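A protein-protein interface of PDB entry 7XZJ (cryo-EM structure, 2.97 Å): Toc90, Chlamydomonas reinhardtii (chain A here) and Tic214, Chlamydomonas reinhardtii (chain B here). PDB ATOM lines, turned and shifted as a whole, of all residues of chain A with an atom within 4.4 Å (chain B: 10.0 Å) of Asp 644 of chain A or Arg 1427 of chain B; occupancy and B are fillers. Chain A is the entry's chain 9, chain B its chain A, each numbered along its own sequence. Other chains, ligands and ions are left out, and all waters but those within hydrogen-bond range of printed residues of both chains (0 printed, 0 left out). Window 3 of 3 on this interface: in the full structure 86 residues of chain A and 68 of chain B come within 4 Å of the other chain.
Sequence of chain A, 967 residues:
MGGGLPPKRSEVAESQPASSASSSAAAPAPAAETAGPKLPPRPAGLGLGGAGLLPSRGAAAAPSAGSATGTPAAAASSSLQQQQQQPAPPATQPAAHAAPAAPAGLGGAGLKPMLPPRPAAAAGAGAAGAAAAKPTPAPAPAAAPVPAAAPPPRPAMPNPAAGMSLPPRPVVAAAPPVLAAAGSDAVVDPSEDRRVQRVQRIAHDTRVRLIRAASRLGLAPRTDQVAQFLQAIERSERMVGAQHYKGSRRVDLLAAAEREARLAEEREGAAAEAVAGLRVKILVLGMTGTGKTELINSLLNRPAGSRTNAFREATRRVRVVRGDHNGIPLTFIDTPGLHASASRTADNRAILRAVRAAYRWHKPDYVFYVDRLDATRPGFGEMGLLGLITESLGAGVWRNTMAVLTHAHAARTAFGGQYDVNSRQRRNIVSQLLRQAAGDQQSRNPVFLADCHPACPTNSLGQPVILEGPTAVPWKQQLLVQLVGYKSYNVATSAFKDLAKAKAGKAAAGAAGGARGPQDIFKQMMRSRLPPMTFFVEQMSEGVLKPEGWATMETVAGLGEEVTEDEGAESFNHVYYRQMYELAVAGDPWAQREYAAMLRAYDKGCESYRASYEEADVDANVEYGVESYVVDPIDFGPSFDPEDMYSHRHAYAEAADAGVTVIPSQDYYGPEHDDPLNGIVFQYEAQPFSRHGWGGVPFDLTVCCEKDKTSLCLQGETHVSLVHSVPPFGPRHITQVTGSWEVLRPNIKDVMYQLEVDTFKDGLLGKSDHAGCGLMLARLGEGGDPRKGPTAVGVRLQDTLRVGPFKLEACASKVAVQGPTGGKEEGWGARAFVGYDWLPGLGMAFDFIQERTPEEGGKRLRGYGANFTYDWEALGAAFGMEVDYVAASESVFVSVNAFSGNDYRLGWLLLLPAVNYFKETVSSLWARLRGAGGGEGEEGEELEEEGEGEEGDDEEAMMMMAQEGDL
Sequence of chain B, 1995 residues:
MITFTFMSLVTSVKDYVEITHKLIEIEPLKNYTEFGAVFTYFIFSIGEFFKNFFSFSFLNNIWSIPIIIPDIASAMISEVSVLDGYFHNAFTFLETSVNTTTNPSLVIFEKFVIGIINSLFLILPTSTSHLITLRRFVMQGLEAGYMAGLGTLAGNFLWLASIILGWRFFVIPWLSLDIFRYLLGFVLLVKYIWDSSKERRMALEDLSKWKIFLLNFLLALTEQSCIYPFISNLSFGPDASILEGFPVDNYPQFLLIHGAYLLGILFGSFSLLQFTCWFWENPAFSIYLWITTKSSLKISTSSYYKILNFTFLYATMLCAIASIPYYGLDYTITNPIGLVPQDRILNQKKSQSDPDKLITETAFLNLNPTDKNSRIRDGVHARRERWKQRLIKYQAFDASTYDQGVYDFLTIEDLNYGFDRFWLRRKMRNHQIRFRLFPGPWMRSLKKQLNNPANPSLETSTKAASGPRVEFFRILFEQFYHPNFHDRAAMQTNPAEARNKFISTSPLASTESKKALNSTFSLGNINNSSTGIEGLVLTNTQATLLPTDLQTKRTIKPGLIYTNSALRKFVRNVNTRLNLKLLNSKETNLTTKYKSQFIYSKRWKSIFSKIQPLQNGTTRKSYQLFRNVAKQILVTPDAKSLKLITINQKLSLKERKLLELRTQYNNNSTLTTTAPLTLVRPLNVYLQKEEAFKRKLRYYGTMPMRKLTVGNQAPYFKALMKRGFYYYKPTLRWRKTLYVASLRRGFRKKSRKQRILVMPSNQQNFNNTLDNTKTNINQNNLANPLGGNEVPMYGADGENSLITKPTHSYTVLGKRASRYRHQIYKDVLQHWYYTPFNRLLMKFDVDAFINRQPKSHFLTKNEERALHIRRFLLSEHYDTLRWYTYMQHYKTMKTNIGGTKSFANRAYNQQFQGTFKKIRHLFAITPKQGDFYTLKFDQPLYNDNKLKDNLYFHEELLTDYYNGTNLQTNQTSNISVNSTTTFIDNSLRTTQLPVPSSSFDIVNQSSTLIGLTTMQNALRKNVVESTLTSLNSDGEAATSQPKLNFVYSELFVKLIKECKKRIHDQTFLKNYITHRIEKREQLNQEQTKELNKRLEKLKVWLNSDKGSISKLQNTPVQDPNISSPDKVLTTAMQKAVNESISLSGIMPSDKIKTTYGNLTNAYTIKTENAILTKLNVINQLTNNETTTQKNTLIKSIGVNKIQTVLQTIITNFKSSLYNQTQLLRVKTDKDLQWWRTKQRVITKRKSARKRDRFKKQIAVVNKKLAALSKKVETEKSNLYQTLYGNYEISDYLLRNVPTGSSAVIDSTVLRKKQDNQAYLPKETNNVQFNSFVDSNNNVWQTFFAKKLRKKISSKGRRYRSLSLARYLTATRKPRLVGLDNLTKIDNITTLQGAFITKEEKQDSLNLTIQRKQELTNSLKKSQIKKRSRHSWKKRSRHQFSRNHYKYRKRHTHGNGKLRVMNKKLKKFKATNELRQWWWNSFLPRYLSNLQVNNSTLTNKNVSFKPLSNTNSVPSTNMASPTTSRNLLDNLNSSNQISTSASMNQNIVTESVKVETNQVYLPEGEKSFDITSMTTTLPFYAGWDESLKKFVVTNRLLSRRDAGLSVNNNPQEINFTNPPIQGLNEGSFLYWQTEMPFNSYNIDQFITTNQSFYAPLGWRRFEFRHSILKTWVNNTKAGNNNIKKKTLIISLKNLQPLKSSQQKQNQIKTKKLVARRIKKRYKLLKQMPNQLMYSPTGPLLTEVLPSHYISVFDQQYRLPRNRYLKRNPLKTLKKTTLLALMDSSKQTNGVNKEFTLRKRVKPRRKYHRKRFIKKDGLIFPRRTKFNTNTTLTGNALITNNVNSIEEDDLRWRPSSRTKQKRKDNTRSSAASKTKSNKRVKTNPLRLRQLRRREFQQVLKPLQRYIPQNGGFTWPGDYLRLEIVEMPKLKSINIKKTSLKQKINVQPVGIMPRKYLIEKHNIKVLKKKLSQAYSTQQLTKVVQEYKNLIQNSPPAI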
ATOM      1  N   PRO A 633      14.063  -9.870 -29.511  1.00  0.00           N
ATOM      2  CA  PRO A 633      15.499 -10.179 -29.443  1.00  0.00           C
ATOM      3  C   PRO A 633      15.825 -11.296 -28.461  1.00  0.00           C
ATOM      4  O   PRO A 633      14.925 -11.911 -27.879  1.00  0.00           O
ATOM      5  CB  PRO A 633      16.124  -8.848 -28.995  1.00  0.00           C
ATOM      6  CG  PRO A 633      15.075  -7.811 -29.239  1.00  0.00           C
ATOM      7  CD  PRO A 633      13.773  -8.509 -29.031  1.00  0.00           C
ATOM      8  N   ILE A 634      17.116 -11.565 -28.273  1.00  0.00           N
ATOM      9  CA  ILE A 634      17.594 -12.634 -27.404  1.00  0.00           C
ATOM     10  C   ILE A 634      18.234 -12.010 -26.173  1.00  0.00           C
ATOM     11  O   ILE A 634      19.114 -11.149 -26.291  1.00  0.00           O
ATOM     12  CB  ILE A 634      18.595 -13.545 -28.132  1.00  0.00           C
ATOM     13  CG1 ILE A 634      18.070 -13.895 -29.523  1.00  0.00           C
ATOM     14  CG2 ILE A 634      18.848 -14.806 -27.323  1.00  0.00           C
ATOM     15  CD1 ILE A 634      19.056 -14.661 -30.364  1.00  0.00           C
ATOM     16  N   PHE A 636      20.632 -11.794 -22.937  1.00  0.00           N
ATOM     17  CA  PHE A 636      21.968 -12.280 -22.618  1.00  0.00           C
ATOM     18  C   PHE A 636      22.408 -12.002 -21.188  1.00  0.00           C
ATOM     19  O   PHE A 636      23.542 -12.341 -20.831  1.00  0.00           O
ATOM     20  CB  PHE A 636      23.000 -11.676 -23.580  1.00  0.00           C
ATOM     21  CG  PHE A 636      22.873 -12.170 -24.987  1.00  0.00           C
ATOM     22  CD1 PHE A 636      22.998 -13.518 -25.273  1.00  0.00           C
ATOM     23  CD2 PHE A 636      22.640 -11.288 -26.026  1.00  0.00           C
ATOM     24  CE1 PHE A 636      22.884 -13.977 -26.567  1.00  0.00           C
ATOM     25  CE2 PHE A 636      22.526 -11.742 -27.322  1.00  0.00           C
ATOM     26  CZ  PHE A 636      22.648 -13.088 -27.593  1.00  0.00           C
ATOM     27  N   PRO A 642      26.138  -1.108 -22.390  1.00  0.00           N
ATOM     28  CA  PRO A 642      24.733  -0.690 -22.310  1.00  0.00           C
ATOM     29  C   PRO A 642      23.739  -1.816 -22.619  1.00  0.00           C
ATOM     30  O   PRO A 642      23.983  -2.574 -23.541  1.00  0.00           O
ATOM     31  CB  PRO A 642      24.639   0.363 -23.421  1.00  0.00           C
ATOM     32  CG  PRO A 642      26.007   0.988 -23.429  1.00  0.00           C
ATOM     33  CD  PRO A 642      26.953  -0.162 -23.152  1.00  0.00           C
ATOM     34  N   GLU A 643      22.641  -1.887 -21.864  1.00  0.00           N
ATOM     35  CA  GLU A 643      21.626  -2.901 -22.114  1.00  0.00           C
ATOM     36  C   GLU A 643      21.084  -2.775 -23.532  1.00  0.00           C
ATOM     37  O   GLU A 643      20.950  -1.675 -24.074  1.00  0.00           O
ATOM     38  CB  GLU A 643      20.490  -2.775 -21.096  1.00  0.00           C
ATOM     39  CG  GLU A 643      19.341  -3.752 -21.293  1.00  0.00           C
ATOM     40  CD  GLU A 643      19.780  -5.199 -21.187  1.00  0.00           C
ATOM     41  OE1 GLU A 643      20.729  -5.485 -20.426  1.00  0.00           O
ATOM     42  OE2 GLU A 643      19.180  -6.052 -21.874  1.00  0.00           O
ATOM     43  N   ASP A 644      20.794  -3.931 -24.138  1.00  0.00           N
ATOM     44  CA  ASP A 644      20.269  -4.032 -25.508  1.00  0.00           C
ATOM     45  C   ASP A 644      21.013  -3.110 -26.473  1.00  0.00           C
ATOM     46  O   ASP A 644      20.423  -2.489 -27.358  1.00  0.00           O
ATOM     47  CB  ASP A 644      18.756  -3.785 -25.554  1.00  0.00           C
ATOM     48  CG  ASP A 644      18.351  -2.433 -24.993  1.00  0.00           C
ATOM     49  OD1 ASP A 644      18.550  -1.413 -25.681  1.00  0.00           O
ATOM     50  OD2 ASP A 644      17.826  -2.389 -23.860  1.00  0.00           O
ATOM     51  N   MET A 645      22.334  -3.032 -26.301  1.00  0.00           N
ATOM     52  CA  MET A 645      23.148  -2.218 -27.197  1.00  0.00           C
ATOM     53  C   MET A 645      23.109  -2.759 -28.622  1.00  0.00           C
ATOM     54  O   MET A 645      23.035  -1.988 -29.586  1.00  0.00           O
ATOM     55  CB  MET A 645      24.584  -2.152 -26.682  1.00  0.00           C
ATOM     56  CG  MET A 645      25.534  -1.379 -27.577  1.00  0.00           C
ATOM     57  SD  MET A 645      27.178  -1.254 -26.852  1.00  0.00           S
ATOM     58  CE  MET A 645      27.549  -2.984 -26.566  1.00  0.00           C
ATOM     59  N   TYR A 646      23.150  -4.083 -28.776  1.00  0.00           N
ATOM     60  CA  TYR A 646      23.147  -4.721 -30.087  1.00  0.00           C
ATOM     61  C   TYR A 646      21.812  -5.383 -30.408  1.00  0.00           C
ATOM     62  O   TYR A 646      21.753  -6.256 -31.278  1.00  0.00           O
ATOM     63  CB  TYR A 646      24.277  -5.748 -30.177  1.00  0.00           C
ATOM     64  CG  TYR A 646      25.660  -5.150 -30.084  1.00  0.00           C
ATOM     65  CD1 TYR A 646      25.952  -3.927 -30.672  1.00  0.00           C
ATOM     66  CD2 TYR A 646      26.674  -5.805 -29.398  1.00  0.00           C
ATOM     67  CE1 TYR A 646      27.217  -3.377 -30.587  1.00  0.00           C
ATOM     68  CE2 TYR A 646      27.942  -5.262 -29.306  1.00  0.00           C
ATOM     69  CZ  TYR A 646      28.208  -4.048 -29.902  1.00  0.00           C
ATOM     70  OH  TYR A 646      29.468  -3.503 -29.812  1.00  0.00           O
ATOM     71  N   SER A 647      20.737  -4.982 -29.726  1.00  0.00           N
ATOM     72  CA  SER A 647      19.442  -5.631 -29.900  1.00  0.00           C
ATOM     73  C   SER A 647      18.909  -5.542 -31.323  1.00  0.00           C
ATOM     74  O   SER A 647      18.038  -6.335 -31.696  1.00  0.00           O
ATOM     75  CB  SER A 647      18.425  -5.017 -28.941  1.00  0.00           C
ATOM     76  OG  SER A 647      18.329  -3.619 -29.147  1.00  0.00           O
ATOM     77  N   HIS A 650      19.436  -8.757 -33.432  1.00  0.00           N
ATOM     78  CA  HIS A 650      18.725  -9.953 -32.997  1.00  0.00           C
ATOM     79  C   HIS A 650      17.222  -9.877 -33.231  1.00  0.00           C
ATOM     80  O   HIS A 650      16.505 -10.811 -32.860  1.00  0.00           O
ATOM     81  CB  HIS A 650      18.997 -10.217 -31.515  1.00  0.00           C
ATOM     82  CG  HIS A 650      20.450 -10.291 -31.175  1.00  0.00           C
ATOM     83  ND1 HIS A 650      21.261 -11.325 -31.592  1.00  0.00           N
ATOM     84  CD2 HIS A 650      21.241  -9.457 -30.462  1.00  0.00           C
ATOM     85  CE1 HIS A 650      22.488 -11.125 -31.146  1.00  0.00           C
ATOM     86  NE2 HIS A 650      22.502  -9.998 -30.457  1.00  0.00           N
ATOM     87  N   GLN B1423       6.811  -2.128 -34.987  1.00  0.00           N
ATOM     88  CA  GLN B1423       8.125  -1.432 -34.917  1.00  0.00           C
ATOM     89  C   GLN B1423       9.165  -2.357 -34.279  1.00  0.00           C
ATOM     90  O   GLN B1423       8.760  -3.267 -33.531  1.00  0.00           O
ATOM     91  CB  GLN B1423       8.005  -0.115 -34.144  1.00  0.00           C
ATOM     92  CG  GLN B1423       7.710  -0.283 -32.660  1.00  0.00           C
ATOM     93  CD  GLN B1423       6.237  -0.424 -32.364  1.00  0.00           C
ATOM     94  OE1 GLN B1423       5.384  -0.126 -33.198  1.00  0.00           O
ATOM     95  NE2 GLN B1423       5.925  -0.878 -31.162  1.00  0.00           N
ATOM     96  N   ILE B1424      10.453  -2.121 -34.550  1.00  0.00           N
ATOM     97  CA  ILE B1424      11.520  -3.038 -34.049  1.00  0.00           C
ATOM     98  C   ILE B1424      11.405  -3.130 -32.525  1.00  0.00           C
ATOM     99  O   ILE B1424      11.265  -2.073 -31.878  1.00  0.00           O
ATOM    100  CB  ILE B1424      12.907  -2.521 -34.480  1.00  0.00           C
ATOM    101  CG1 ILE B1424      12.931  -2.120 -35.957  1.00  0.00           C
ATOM    102  CG2 ILE B1424      13.996  -3.530 -34.150  1.00  0.00           C
ATOM    103  CD1 ILE B1424      12.718  -3.270 -36.912  1.00  0.00           C
ATOM    104  N   LYS B1425      11.479  -4.346 -31.978  1.00  0.00           N
ATOM    105  CA  LYS B1425      11.292  -4.535 -30.515  1.00  0.00           C
ATOM    106  C   LYS B1425      12.630  -4.365 -29.794  1.00  0.00           C
ATOM    107  O   LYS B1425      13.663  -4.754 -30.374  1.00  0.00           O
ATOM    108  CB  LYS B1425      10.695  -5.916 -30.227  1.00  0.00           C
ATOM    109  CG  LYS B1425       9.417  -6.248 -30.986  1.00  0.00           C
ATOM    110  CD  LYS B1425       8.294  -5.264 -30.737  1.00  0.00           C
ATOM    111  CE  LYS B1425       7.065  -5.551 -31.574  1.00  0.00           C
ATOM    112  NZ  LYS B1425       6.111  -4.416 -31.553  1.00  0.00           N
ATOM    113  N   LYS B1426      12.606  -3.803 -28.582  1.00  0.00           N
ATOM    114  CA  LYS B1426      13.816  -3.616 -27.798  1.00  0.00           C
ATOM    115  C   LYS B1426      13.657  -4.313 -26.456  1.00  0.00           C
ATOM    116  O   LYS B1426      12.554  -4.394 -25.909  1.00  0.00           O
ATOM    117  CB  LYS B1426      14.117  -2.130 -27.576  1.00  0.00           C
ATOM    118  CG  LYS B1426      14.181  -1.298 -28.843  1.00  0.00           C
ATOM    119  CD  LYS B1426      15.335  -1.719 -29.731  1.00  0.00           C
ATOM    120  CE  LYS B1426      15.426  -0.826 -30.959  1.00  0.00           C
ATOM    121  NZ  LYS B1426      16.568  -1.193 -31.842  1.00  0.00           N
ATOM    122  N   ARG B1427      14.768  -4.823 -25.932  1.00  0.00           N
ATOM    123  CA  ARG B1427      14.741  -5.475 -24.633  1.00  0.00           C
ATOM    124  C   ARG B1427      14.376  -4.473 -23.544  1.00  0.00           C
ATOM    125  O   ARG B1427      14.386  -3.255 -23.752  1.00  0.00           O
ATOM    126  CB  ARG B1427      16.091  -6.121 -24.330  1.00  0.00           C
ATOM    127  CG  ARG B1427      16.652  -6.946 -25.474  1.00  0.00           C
ATOM    128  CD  ARG B1427      18.012  -7.516 -25.117  1.00  0.00           C
ATOM    129  NE  ARG B1427      18.827  -7.759 -26.299  1.00  0.00           N
ATOM    130  CZ  ARG B1427      20.096  -8.149 -26.269  1.00  0.00           C
ATOM    131  NH1 ARG B1427      20.726  -8.365 -25.127  1.00  0.00           N
ATOM    132  NH2 ARG B1427      20.747  -8.322 -27.414  1.00  0.00           N
ATOM    133  N   SER B1428      14.040  -5.007 -22.373  1.00  0.00           N
ATOM    134  CA  SER B1428      13.533  -4.308 -21.193  1.00  0.00           C
ATOM    135  C   SER B1428      12.081  -3.894 -21.393  1.00  0.00           C
ATOM    136  O   SER B1428      11.513  -3.247 -20.507  1.00  0.00           O
ATOM    137  CB  SER B1428      14.360  -3.077 -20.794  1.00  0.00           C
ATOM    138  OG  SER B1428      14.180  -2.019 -21.718  1.00  0.00           O
ATOM    139  N   ARG B1429      11.464  -4.231 -22.524  1.00  0.00           N
ATOM    140  CA  ARG B1429      10.047  -3.956 -22.707  1.00  0.00           C
ATOM    141  C   ARG B1429       9.221  -4.848 -21.790  1.00  0.00           C
ATOM    142  O   ARG B1429       9.539  -6.024 -21.589  1.00  0.00           O
ATOM    143  CB  ARG B1429       9.643  -4.175 -24.164  1.00  0.00           C
ATOM    144  CG  ARG B1429       9.856  -5.595 -24.668  1.00  0.00           C
ATOM    145  CD  ARG B1429       9.649  -5.688 -26.170  1.00  0.00           C
ATOM    146  NE  ARG B1429       8.259  -5.485 -26.554  1.00  0.00           N
ATOM    147  CZ  ARG B1429       7.386  -6.468 -26.748  1.00  0.00           C
ATOM    148  NH1 ARG B1429       7.726  -7.736 -26.587  1.00  0.00           N
ATOM    149  NH2 ARG B1429       6.145  -6.168 -27.115  1.00  0.00           N
ATOM    150  N   HIS B1430       8.159  -4.275 -21.229  1.00  0.00           N
ATOM    151  CA  HIS B1430       7.238  -4.999 -20.359  1.00  0.00           C
ATOM    152  C   HIS B1430       7.982  -5.684 -19.215  1.00  0.00           C
ATOM    153  O   HIS B1430       7.792  -6.870 -18.934  1.00  0.00           O
ATOM    154  CB  HIS B1430       6.410  -6.003 -21.159  1.00  0.00           C
ATOM    155  CG  HIS B1430       5.754  -5.414 -22.370  1.00  0.00           C
ATOM    156  ND1 HIS B1430       4.797  -4.425 -22.290  1.00  0.00           N
ATOM    157  CD2 HIS B1430       5.916  -5.674 -23.688  1.00  0.00           C
ATOM    158  CE1 HIS B1430       4.400  -4.100 -23.507  1.00  0.00           C
ATOM    159  NE2 HIS B1430       5.063  -4.844 -24.374  1.00  0.00           N
ATOM    160  N   SER B1431       8.872  -4.920 -18.572  1.00  0.00           N
ATOM    161  CA  SER B1431       9.694  -5.473 -17.463  1.00  0.00           C
ATOM    162  C   SER B1431       8.791  -6.030 -16.362  1.00  0.00           C
ATOM    163  O   SER B1431       9.025  -7.178 -15.932  1.00  0.00           O
ATOM    164  CB  SER B1431      10.626  -4.423 -16.922  1.00  0.00           C
ATOM    165  OG  SER B1431       9.905  -3.275 -16.501  1.00  0.00           O
ATOM    166  N   LYS B1434       7.106  -9.384 -17.327  1.00  0.00           N
ATOM    167  CA  LYS B1434       7.951 -10.606 -17.325  1.00  0.00           C
ATOM    168  C   LYS B1434       8.213 -11.042 -15.882  1.00  0.00           C
ATOM    169  O   LYS B1434       8.089 -12.248 -15.598  1.00  0.00           O
ATOM    170  CB  LYS B1434       9.271 -10.346 -18.054  1.00  0.00           C
ATOM    171  CG  LYS B1434       9.137  -9.909 -19.507  1.00  0.00           C
ATOM    172  CD  LYS B1434      10.456  -9.887 -20.248  1.00  0.00           C
ATOM    173  CE  LYS B1434      11.487  -8.981 -19.609  1.00  0.00           C
ATOM    174  NZ  LYS B1434      11.128  -7.551 -19.751  1.00  0.00           N
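O of Ile 634 of chain A lies close to NE of Arg 1427 of chain B, at 3.4 Å.
The backbone carbonyl oxygen (O) of Asp 644 of chain A sits at hydrogen-bond distance from the side-chain hydroxyl (OG) of Ser 647 of chain A (3.0 Å).
CG of Pro 633 of chain A touches O of Lys 1425 of chain B (3.6 Å).
NE of Arg 1427 of chain B touches CB of Pro 633 of chain A (3.97 Å).
Arg 1427 of chain B touches Phe 636 of chain A (NH1 to CD2, 3.6 Å).
CD of Arg 1427 of chain B touches OE2 of Glu 643 of chain A, 3.7 Å away.
Asp 644 of chain A touches Arg 1427 of chain B (OD2 to O, 3.5 Å).
Ser 647 of chain A touches Lys 1426 of chain B (OG to CD, 3.6 Å).
CB of Ser 647 of chain A touches NE of Arg 1427 of chain B, at 3.8 Å.
His 650 of chain A touches Arg 1427 of chain B.
Of chain B, only Arg 1427 (3.5 Å) comes within 4 Å of Asp 644 of chain A.
Of chain B, only Lys 1425 (3.6 Å) and Arg 1427 (3.97 Å) come within 4 Å of Pro 633 of chain A.
Glu 643 of chain A touches just one residue of chain B: Arg 1427.
Of chain B, only Lys 1426 (3.6 Å) and Arg 1427 (3.8 Å) come within 4 Å of Ser 647 of chain A.
Of the printed residues of chain A, Lys 1426 of chain B touches Ser 647 (3.6 Å).
Printed residues of chain B within 4 Å of His 650 of chain A: Arg 1427.
The nearest residue of chain B that does not touch Asp 644 of chain A is Ser 1428 of chain B (4.2 Å).
The nearest printed residue of chain A that does not touch Lys 1426 of chain B is Pro 633 of chain A (4.6 Å).
Of the 10 printed residues of chain A, 7 touch a printed residue of chain B.
Hydrophobic or aromatic side chains of chain A that line the printed part of chain B: Pro 633, Phe 636 and His 650.
Among the printed residues, no Asp or Glu carboxylate lies within 4 Å of a Lys or Arg side-chain nitrogen of the other chain.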
